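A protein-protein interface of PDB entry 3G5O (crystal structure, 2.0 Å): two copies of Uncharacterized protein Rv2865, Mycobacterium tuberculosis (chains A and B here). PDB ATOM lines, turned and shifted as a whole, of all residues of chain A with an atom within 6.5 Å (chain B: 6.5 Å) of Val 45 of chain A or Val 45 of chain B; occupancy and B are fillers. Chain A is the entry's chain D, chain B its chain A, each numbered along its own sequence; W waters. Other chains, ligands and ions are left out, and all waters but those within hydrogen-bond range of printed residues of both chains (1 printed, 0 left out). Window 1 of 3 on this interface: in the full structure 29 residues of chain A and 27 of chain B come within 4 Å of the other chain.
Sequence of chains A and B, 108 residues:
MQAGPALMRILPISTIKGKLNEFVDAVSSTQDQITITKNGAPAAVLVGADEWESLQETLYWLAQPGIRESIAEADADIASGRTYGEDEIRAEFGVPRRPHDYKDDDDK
Gln 33 of chain A touches Trp 52 of chain B, and with the chains exchanged Trp 52 of chain A touches Gln 33 of chain B. Ala 44 of chain A touches Val 47 of chain B, and with the chains exchanged Val 47 of chain A touches Ala 44 of chain B. Val 45 of chain A touches Leu 46 of chain B, and with the chains exchanged Leu 46 of chain A touches Val 45 of chain B. Leu 46 of chain A touches Ile 36 of chain B, but with the chains exchanged Ile 36 of chain A does not touch Leu 46 of chain B (4.01 Å).
Ala 43 of chain A touches Gly 48 of chain B. Val 27 of chain B touches Ala 44 of chain A. Leu 46 of chain B touches Ala 44 of chain A (CD1 to CB, 3.8 Å). CA of Ala 44 of chain A touches O of Val 47 of chain B, 3.2 Å away. CB of Trp 52 of chain B touches CG2 of Val 45 of chain A, at 3.7 Å. CA of Ala 44 of chain B touches O of Val 47 of chain A, at 3.1 Å. CG1 of Val 47 of chain A touches CH2 of Trp 52 of chain B, 3.8 Å away. Ala 44 of chain B touches Ala 49 of chain A. Trp 52 of chain A touches Val 45 of chain B. CH2 of Trp 52 of chain A touches CG1 of Val 47 of chain B, at 3.7 Å.
The backbone carbonyl oxygen (O) of Ala 43 of chain B sits at hydrogen-bond distance from the backbone NH (N) of Ala 49 of chain A (3.0 Å). O of Val 47 of chain A sits at hydrogen-bond distance from N of Val 45 of chain B. N of Val 45 of chain A lies within hydrogen-bond range of O of Val 47 of chain B (2.7 Å). The backbone carbonyl oxygen (O) of Ala 43 of chain A lies within hydrogen-bond range of the backbone NH (N) of Ala 49 of chain B (3.0 Å).
N of Gly 48 of chain B sits close to O of Val 27 of chain B (3.5 Å). The backbone NH of Leu 46 of chain B is in hydrogen-bond range of the backbone carbonyl oxygen of Ile 34 of chain B (2.8 Å). The backbone carbonyl oxygen (O) of Ile 36 of chain B sits at hydrogen-bond distance from the backbone NH (N) of Ala 43 of chain B. N of Ile 36 of chain B sits at hydrogen-bond distance from O of Ala 44 of chain B, at 2.7 Å. The side-chain sulfur of Met 8 of chain A is in hydrogen-bond range of the side-chain hydroxyl of Thr 35 of chain A, at 2.8 Å. The backbone carbonyl oxygen of Ile 36 of chain A lies within hydrogen-bond range of the backbone NH of Ala 43 of chain A (2.7 Å).
Of chain B, only Val 45 (3.5 Å), Leu 46 (3.4 Å), Val 47 (2.7 Å) and Trp 52 (3.7 Å) come within 4 Å of Val 45 of chain A. Of chain A, only Val 45 (3.5 Å), Leu 46 (3.4 Å), Val 47 (2.8 Å) and Trp 52 (3.6 Å) come within 4 Å of Val 45 of chain B. Of the printed residues of chain A, Ala 43 of chain B touches Gly 48 (3.6 Å) and Ala 49 (3.0 Å). Of the printed residues of chain A, Ala 49 of chain B touches Ala 43 (3.0 Å) and Ala 44 (3.6 Å). Glu 53 of chain A touches none of the printed residues of chain B. Ile 34 of chain B touches none of the printed residues of chain A. The nearest residue of chain B that does not touch Val 45 of chain A is Ala 49 of chain B (4.1 Å).
Printed residues of chain A that touch a printed residue of chain B: Met 8, Val 27, Gln 33, Ala 43, Ala 44, Val 45, Leu 46, Val 47, Gly 48, Ala 49 and Trp 52. Printed residues of chain B that touch a printed residue of chain A: Val 27, Gln 33, Ile 36, Ala 43, Ala 44, Val 45, Leu 46, Val 47, Gly 48, Ala 49 and Trp 52. Hydrophobic or aromatic side chains of chain B within 4 Å of the printed part of chain A: Val 27, Ile 36, Ala 44, Val 45, Leu 46, Val 47, Ala 49 and Trp 52. Along chain B the printed residues that touch a printed residue of chain A span positions 27 to 52. Among the printed residues, no Asp or Glu carboxylate lies within 4 Å of a Lys or Arg side-chain nitrogen of the other chain.
Water W1 lies within hydrogen-bond range of the backbone NH (N) of Asp 50 of chain B, the backbone NH (N) of Ala 49 of chain B and the backbone carbonyl oxygen (O) of Ala 43 of chain A.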
ATOM      1  N   MET A   8       4.254  -4.654  -6.478  1.00  0.00           N
ATOM      2  CA  MET A   8       4.153  -4.720  -5.001  1.00  0.00           C
ATOM      3  C   MET A   8       3.997  -6.172  -4.550  1.00  0.00           C
ATOM      4  O   MET A   8       3.078  -6.868  -4.969  1.00  0.00           O
ATOM      5  CB  MET A   8       3.015  -3.840  -4.455  1.00  0.00           C
ATOM      6  CG  MET A   8       2.705  -3.972  -2.892  1.00  0.00           C
ATOM      7  SD  MET A   8       3.945  -3.347  -1.664  1.00  0.00           S
ATOM      8  CE  MET A   8       3.733  -1.547  -1.809  1.00  0.00           C
ATOM      9  N   VAL A  27      15.141  -4.690  -4.210  1.00  0.00           N
ATOM     10  CA  VAL A  27      14.451  -3.393  -4.369  1.00  0.00           C
ATOM     11  C   VAL A  27      15.363  -2.264  -4.820  1.00  0.00           C
ATOM     12  O   VAL A  27      14.895  -1.370  -5.496  1.00  0.00           O
ATOM     13  CB  VAL A  27      13.625  -2.931  -3.125  1.00  0.00           C
ATOM     14  CG1 VAL A  27      12.526  -3.927  -2.805  1.00  0.00           C
ATOM     15  CG2 VAL A  27      14.529  -2.681  -1.880  1.00  0.00           C
ATOM     16  N   GLN A  33       8.279  -2.844  -4.703  1.00  0.00           N
ATOM     17  CA  GLN A  33       8.064  -2.555  -3.311  1.00  0.00           C
ATOM     18  C   GLN A  33       7.696  -3.838  -2.624  1.00  0.00           C
ATOM     19  O   GLN A  33       7.069  -4.723  -3.233  1.00  0.00           O
ATOM     20  CB  GLN A  33       6.936  -1.544  -3.140  1.00  0.00           C
ATOM     21  CG  GLN A  33       7.082  -0.341  -4.052  1.00  0.00           C
ATOM     22  CD  GLN A  33       5.753   0.146  -4.588  1.00  0.00           C
ATOM     23  OE1 GLN A  33       4.707  -0.014  -3.937  1.00  0.00           O
ATOM     24  NE2 GLN A  33       5.780   0.751  -5.775  1.00  0.00           N
ATOM     25  N   ILE A  34       8.094  -3.923  -1.364  1.00  0.00           N
ATOM     26  CA  ILE A  34       7.748  -5.035  -0.519  1.00  0.00           C
ATOM     27  C   ILE A  34       7.017  -4.501   0.690  1.00  0.00           C
ATOM     28  O   ILE A  34       7.541  -3.669   1.431  1.00  0.00           O
ATOM     29  CB  ILE A  34       8.969  -5.844  -0.083  1.00  0.00           C
ATOM     30  CG1 ILE A  34       9.623  -6.482  -1.320  1.00  0.00           C
ATOM     31  CG2 ILE A  34       8.568  -6.937   0.952  1.00  0.00           C
ATOM     32  CD1 ILE A  34      11.068  -6.821  -1.077  1.00  0.00           C
ATOM     33  N   THR A  35       5.801  -4.982   0.884  1.00  0.00           N
ATOM     34  CA  THR A  35       5.098  -4.729   2.139  1.00  0.00           C
ATOM     35  C   THR A  35       5.376  -5.889   3.060  1.00  0.00           C
ATOM     36  O   THR A  35       5.116  -7.030   2.730  1.00  0.00           O
ATOM     37  CB  THR A  35       3.573  -4.569   1.911  1.00  0.00           C
ATOM     38  OG1 THR A  35       3.355  -3.414   1.085  1.00  0.00           O
ATOM     39  CG2 THR A  35       2.847  -4.398   3.230  1.00  0.00           C
ATOM     40  N   ILE A  36       5.909  -5.601   4.227  1.00  0.00           N
ATOM     41  CA  ILE A  36       6.238  -6.656   5.187  1.00  0.00           C
ATOM     42  C   ILE A  36       5.120  -6.778   6.203  1.00  0.00           C
ATOM     43  O   ILE A  36       4.731  -5.776   6.809  1.00  0.00           O
ATOM     44  CB  ILE A  36       7.542  -6.311   5.917  1.00  0.00           C
ATOM     45  CG1 ILE A  36       8.691  -6.203   4.895  1.00  0.00           C
ATOM     46  CG2 ILE A  36       7.855  -7.408   6.939  1.00  0.00           C
ATOM     47  CD1 ILE A  36       9.956  -5.561   5.437  1.00  0.00           C
ATOM     48  N   ALA A  43       3.079  -4.045   8.058  1.00  0.00           N
ATOM     49  CA  ALA A  43       3.760  -3.294   9.118  1.00  0.00           C
ATOM     50  C   ALA A  43       4.692  -2.263   8.519  1.00  0.00           C
ATOM     51  O   ALA A  43       4.804  -1.166   9.035  1.00  0.00           O
ATOM     52  CB  ALA A  43       4.549  -4.235  10.069  1.00  0.00           C
ATOM     53  N   ALA A  44       5.385  -2.627   7.444  1.00  0.00           N
ATOM     54  CA  ALA A  44       6.385  -1.749   6.894  1.00  0.00           C
ATOM     55  C   ALA A  44       6.467  -1.923   5.393  1.00  0.00           C
ATOM     56  O   ALA A  44       6.021  -2.934   4.845  1.00  0.00           O
ATOM     57  CB  ALA A  44       7.783  -2.074   7.519  1.00  0.00           C
ATOM     58  N   VAL A  45       7.037  -0.929   4.735  1.00  0.00           N
ATOM     59  CA  VAL A  45       7.260  -1.026   3.305  1.00  0.00           C
ATOM     60  C   VAL A  45       8.728  -0.766   3.052  1.00  0.00           C
ATOM     61  O   VAL A  45       9.308   0.203   3.592  1.00  0.00           O
ATOM     62  CB  VAL A  45       6.352  -0.043   2.512  1.00  0.00           C
ATOM     63  CG1 VAL A  45       6.755   0.005   1.045  1.00  0.00           C
ATOM     64  CG2 VAL A  45       4.869  -0.424   2.636  1.00  0.00           C
ATOM     65  N   LEU A  46       9.328  -1.645   2.248  1.00  0.00           N
ATOM     66  CA  LEU A  46      10.702  -1.516   1.777  1.00  0.00           C
ATOM     67  C   LEU A  46      10.754  -1.139   0.269  1.00  0.00           C
ATOM     68  O   LEU A  46      10.146  -1.815  -0.551  1.00  0.00           O
ATOM     69  CB  LEU A  46      11.437  -2.850   1.990  1.00  0.00           C
ATOM     70  CG  LEU A  46      12.965  -2.953   1.716  1.00  0.00           C
ATOM     71  CD1 LEU A  46      13.785  -2.172   2.761  1.00  0.00           C
ATOM     72  CD2 LEU A  46      13.485  -4.415   1.686  1.00  0.00           C
ATOM     73  N   VAL A  47      11.481  -0.078  -0.085  1.00  0.00           N
ATOM     74  CA  VAL A  47      11.697   0.258  -1.498  1.00  0.00           C
ATOM     75  C   VAL A  47      13.154   0.618  -1.723  1.00  0.00           C
ATOM     76  O   VAL A  47      13.878   0.908  -0.788  1.00  0.00           O
ATOM     77  CB  VAL A  47      10.819   1.476  -1.967  1.00  0.00           C
ATOM     78  CG1 VAL A  47       9.350   1.141  -1.845  1.00  0.00           C
ATOM     79  CG2 VAL A  47      11.146   2.734  -1.167  1.00  0.00           C
ATOM     80  N   GLY A  48      13.573   0.635  -2.984  1.00  0.00           N
ATOM     81  CA  GLY A  48      14.911   1.053  -3.319  1.00  0.00           C
ATOM     82  C   GLY A  48      15.137   2.520  -2.962  1.00  0.00           C
ATOM     83  O   GLY A  48      14.192   3.310  -2.925  1.00  0.00           O
ATOM     84  N   ALA A  49      16.386   2.856  -2.651  1.00  0.00           N
ATOM     85  CA  ALA A  49      16.783   4.236  -2.433  1.00  0.00           C
ATOM     86  C   ALA A  49      16.442   5.135  -3.630  1.00  0.00           C
ATOM     87  O   ALA A  49      15.966   6.263  -3.445  1.00  0.00           O
ATOM     88  CB  ALA A  49      18.283   4.317  -2.131  1.00  0.00           C
ATOM     89  N   TRP A  52      12.748   5.754  -3.677  1.00  0.00           N
ATOM     90  CA  TRP A  52      12.381   6.702  -2.639  1.00  0.00           C
ATOM     91  C   TRP A  52      12.663   8.126  -3.126  1.00  0.00           C
ATOM     92  O   TRP A  52      11.833   9.022  -2.930  1.00  0.00           O
ATOM     93  CB  TRP A  52      13.152   6.436  -1.367  1.00  0.00           C
ATOM     94  CG  TRP A  52      12.771   7.316  -0.249  1.00  0.00           C
ATOM     95  CD1 TRP A  52      13.495   8.369   0.256  1.00  0.00           C
ATOM     96  CD2 TRP A  52      11.579   7.236   0.535  1.00  0.00           C
ATOM     97  NE1 TRP A  52      12.827   8.931   1.308  1.00  0.00           N
ATOM     98  CE2 TRP A  52      11.653   8.259   1.508  1.00  0.00           C
ATOM     99  CE3 TRP A  52      10.458   6.391   0.517  1.00  0.00           C
ATOM    100  CZ2 TRP A  52      10.633   8.492   2.430  1.00  0.00           C
ATOM    101  CZ3 TRP A  52       9.446   6.610   1.444  1.00  0.00           C
ATOM    102  CH2 TRP A  52       9.542   7.650   2.391  1.00  0.00           C
ATOM    103  N   GLU A  53      13.828   8.334  -3.730  1.00  0.00           N
ATOM    104  CA  GLU A  53      14.172   9.660  -4.268  1.00  0.00           C
ATOM    105  C   GLU A  53      13.191  10.090  -5.359  1.00  0.00           C
ATOM    106  O   GLU A  53      12.819  11.256  -5.425  1.00  0.00           O
ATOM    107  CB  GLU A  53      15.602   9.637  -4.867  1.00  0.00           C
ATOM    108  CG  GLU A  53      16.684   9.693  -3.789  1.00  0.00           C
ATOM    109  CD  GLU A  53      16.623  11.024  -3.031  1.00  0.00           C
ATOM    110  OE1 GLU A  53      16.901  12.073  -3.677  1.00  0.00           O
ATOM    111  OE2 GLU A  53      16.247  11.031  -1.824  1.00  0.00           O
ATOM    112  N   VAL B  27       9.137   1.671  12.722  1.00  0.00           N
ATOM    113  CA  VAL B  27       8.579   2.471  11.643  1.00  0.00           C
ATOM    114  C   VAL B  27       7.049   2.268  11.517  1.00  0.00           C
ATOM    115  O   VAL B  27       6.321   3.171  11.104  1.00  0.00           O
ATOM    116  CB  VAL B  27       9.291   2.242  10.285  1.00  0.00           C
ATOM    117  CG1 VAL B  27      10.783   2.458  10.429  1.00  0.00           C
ATOM    118  CG2 VAL B  27       8.979   0.870   9.720  1.00  0.00           C
ATOM    119  N   GLN B  33      11.724   7.041   9.252  1.00  0.00           N
ATOM    120  CA  GLN B  33      12.263   6.314   8.112  1.00  0.00           C
ATOM    121  C   GLN B  33      13.670   5.873   8.364  1.00  0.00           C
ATOM    122  O   GLN B  33      14.429   6.556   9.051  1.00  0.00           O
ATOM    123  CB  GLN B  33      12.251   7.133   6.835  1.00  0.00           C
ATOM    124  CG  GLN B  33      12.122   8.587   7.087  1.00  0.00           C
ATOM    125  CD  GLN B  33      12.024   9.358   5.776  1.00  0.00           C
ATOM    126  OE1 GLN B  33      11.109  10.156   5.588  1.00  0.00           O
ATOM    127  NE2 GLN B  33      12.973   9.113   4.872  1.00  0.00           N
ATOM    128  N   ILE B  34      14.016   4.748   7.772  1.00  0.00           N
ATOM    129  CA  ILE B  34      15.369   4.233   7.832  1.00  0.00           C
ATOM    130  C   ILE B  34      15.875   4.101   6.419  1.00  0.00           C
ATOM    131  O   ILE B  34      15.263   3.408   5.609  1.00  0.00           O
ATOM    132  CB  ILE B  34      15.392   2.842   8.443  1.00  0.00           C
ATOM    133  CG1 ILE B  34      14.721   2.852   9.816  1.00  0.00           C
ATOM    134  CG2 ILE B  34      16.850   2.316   8.507  1.00  0.00           C
ATOM    135  CD1 ILE B  34      14.522   1.471  10.384  1.00  0.00           C
ATOM    136  N   THR B  35      16.966   4.791   6.104  1.00  0.00           N
ATOM    137  CA  THR B  35      17.711   4.514   4.891  1.00  0.00           C
ATOM    138  C   THR B  35      18.753   3.462   5.256  1.00  0.00           C
ATOM    139  O   THR B  35      19.569   3.644   6.209  1.00  0.00           O
ATOM    140  CB  THR B  35      18.427   5.759   4.342  1.00  0.00           C
ATOM    141  OG1 THR B  35      17.486   6.798   4.078  1.00  0.00           O
ATOM    142  CG2 THR B  35      19.200   5.439   3.050  1.00  0.00           C
ATOM    143  N   ILE B  36      18.731   2.375   4.495  1.00  0.00           N
ATOM    144  CA  ILE B  36      19.537   1.234   4.773  1.00  0.00           C
ATOM    145  C   ILE B  36      20.682   1.308   3.782  1.00  0.00           C
ATOM    146  O   ILE B  36      20.440   1.369   2.578  1.00  0.00           O
ATOM    147  CB  ILE B  36      18.742  -0.076   4.561  1.00  0.00           C
ATOM    148  CG1 ILE B  36      17.614  -0.215   5.603  1.00  0.00           C
ATOM    149  CG2 ILE B  36      19.674  -1.284   4.610  1.00  0.00           C
ATOM    150  CD1 ILE B  36      16.724  -1.451   5.355  1.00  0.00           C
ATOM    151  N   ALA B  43      20.789   2.113  -0.131  1.00  0.00           N
ATOM    152  CA  ALA B  43      20.305   1.064  -1.023  1.00  0.00           C
ATOM    153  C   ALA B  43      18.798   0.876  -0.991  1.00  0.00           C
ATOM    154  O   ALA B  43      18.204   0.529  -2.007  1.00  0.00           O
ATOM    155  CB  ALA B  43      21.020  -0.294  -0.736  1.00  0.00           C
ATOM    156  N   ALA B  44      18.191   1.101   0.172  1.00  0.00           N
ATOM    157  CA  ALA B  44      16.751   0.929   0.355  1.00  0.00           C
ATOM    158  C   ALA B  44      16.289   1.832   1.465  1.00  0.00           C
ATOM    159  O   ALA B  44      17.104   2.330   2.297  1.00  0.00           O
ATOM    160  CB  ALA B  44      16.406  -0.515   0.712  1.00  0.00           C
ATOM    161  N   VAL B  45      14.973   1.999   1.527  1.00  0.00           N
ATOM    162  CA  VAL B  45      14.376   2.791   2.565  1.00  0.00           C
ATOM    163  C   VAL B  45      13.255   1.943   3.166  1.00  0.00           C
ATOM    164  O   VAL B  45      12.480   1.282   2.436  1.00  0.00           O
ATOM    165  CB  VAL B  45      13.823   4.155   2.004  1.00  0.00           C
ATOM    166  CG1 VAL B  45      13.037   4.880   3.075  1.00  0.00           C
ATOM    167  CG2 VAL B  45      14.967   5.041   1.513  1.00  0.00           C
ATOM    168  N   LEU B  46      13.174   1.968   4.496  1.00  0.00           N
ATOM    169  CA  LEU B  46      12.070   1.323   5.199  1.00  0.00           C
ATOM    170  C   LEU B  46      11.184   2.346   5.895  1.00  0.00           C
ATOM    171  O   LEU B  46      11.695   3.196   6.628  1.00  0.00           O
ATOM    172  CB  LEU B  46      12.623   0.302   6.226  1.00  0.00           C
ATOM    173  CG  LEU B  46      11.669  -0.669   6.913  1.00  0.00           C
ATOM    174  CD1 LEU B  46      11.270  -1.816   5.981  1.00  0.00           C
ATOM    175  CD2 LEU B  46      12.348  -1.246   8.170  1.00  0.00           C
ATOM    176  N   VAL B  47       9.860   2.260   5.684  1.00  0.00           N
ATOM    177  CA  VAL B  47       8.898   3.134   6.367  1.00  0.00           C
ATOM    178  C   VAL B  47       7.691   2.325   6.821  1.00  0.00           C
ATOM    179  O   VAL B  47       7.506   1.214   6.370  1.00  0.00           O
ATOM    180  CB  VAL B  47       8.386   4.297   5.445  1.00  0.00           C
ATOM    181  CG1 VAL B  47       9.518   5.206   5.112  1.00  0.00           C
ATOM    182  CG2 VAL B  47       7.746   3.748   4.166  1.00  0.00           C
ATOM    183  N   GLY B  48       6.852   2.891   7.694  1.00  0.00           N
ATOM    184  CA  GLY B  48       5.642   2.188   8.160  1.00  0.00           C
ATOM    185  C   GLY B  48       4.706   1.961   6.980  1.00  0.00           C
ATOM    186  O   GLY B  48       4.718   2.743   5.990  1.00  0.00           O
ATOM    187  N   ALA B  49       3.905   0.902   7.050  1.00  0.00           N
ATOM    188  CA  ALA B  49       2.852   0.717   6.065  1.00  0.00           C
ATOM    189  C   ALA B  49       1.831   1.866   6.037  1.00  0.00           C
ATOM    190  O   ALA B  49       1.393   2.300   4.936  1.00  0.00           O
ATOM    191  CB  ALA B  49       2.129  -0.655   6.273  1.00  0.00           C
ATOM    192  N   ASP B  50       1.421   2.342   7.214  1.00  0.00           N
ATOM    193  CA  ASP B  50       0.515   3.482   7.315  1.00  0.00           C
ATOM    194  C   ASP B  50       1.199   4.726   6.730  1.00  0.00           C
ATOM    195  O   ASP B  50       0.585   5.490   5.983  1.00  0.00           O
ATOM    196  CB  ASP B  50       0.094   3.756   8.754  1.00  0.00           C
ATOM    197  CG  ASP B  50      -0.797   2.669   9.332  1.00  0.00           C
ATOM    198  OD1 ASP B  50      -1.422   1.901   8.563  1.00  0.00           O
ATOM    199  OD2 ASP B  50      -0.884   2.597  10.573  1.00  0.00           O
ATOM    200  N   TRP B  52       3.457   4.791   4.396  1.00  0.00           N
ATOM    201  CA  TRP B  52       3.499   4.605   2.952  1.00  0.00           C
ATOM    202  C   TRP B  52       2.141   5.000   2.327  1.00  0.00           C
ATOM    203  O   TRP B  52       2.101   5.737   1.351  1.00  0.00           O
ATOM    204  CB  TRP B  52       3.829   3.150   2.615  1.00  0.00           C
ATOM    205  CG  TRP B  52       3.866   2.903   1.134  1.00  0.00           C
ATOM    206  CD1 TRP B  52       2.894   2.312   0.355  1.00  0.00           C
ATOM    207  CD2 TRP B  52       4.908   3.291   0.262  1.00  0.00           C
ATOM    208  NE1 TRP B  52       3.303   2.295  -0.962  1.00  0.00           N
ATOM    209  CE2 TRP B  52       4.544   2.871  -1.042  1.00  0.00           C
ATOM    210  CE3 TRP B  52       6.136   3.943   0.455  1.00  0.00           C
ATOM    211  CZ2 TRP B  52       5.363   3.093  -2.163  1.00  0.00           C
ATOM    212  CZ3 TRP B  52       6.983   4.140  -0.672  1.00  0.00           C
ATOM    213  CH2 TRP B  52       6.571   3.705  -1.963  1.00  0.00           C
ATOM    214  N   GLU B  53       1.054   4.575   2.948  1.00  0.00           N
ATOM    215  CA  GLU B  53      -0.307   4.975   2.535  1.00  0.00           C
ATOM    216  C   GLU B  53      -0.511   6.521   2.603  1.00  0.00           C
ATOM    217  O   GLU B  53      -1.007   7.124   1.643  1.00  0.00           O
ATOM    218  CB  GLU B  53      -1.336   4.280   3.417  1.00  0.00           C
ATOM    219  CG  GLU B  53      -1.767   2.959   2.896  1.00  0.00           C
ATOM    220  CD  GLU B  53      -2.508   3.153   1.554  1.00  0.00           C
ATOM    221  OE1 GLU B  53      -3.557   3.842   1.528  1.00  0.00           O
ATOM    222  OE2 GLU B  53      -2.003   2.666   0.524  1.00  0.00           O
HETATM  223  O   HOH W   1       2.207   0.933   9.652  1.00  0.00           O
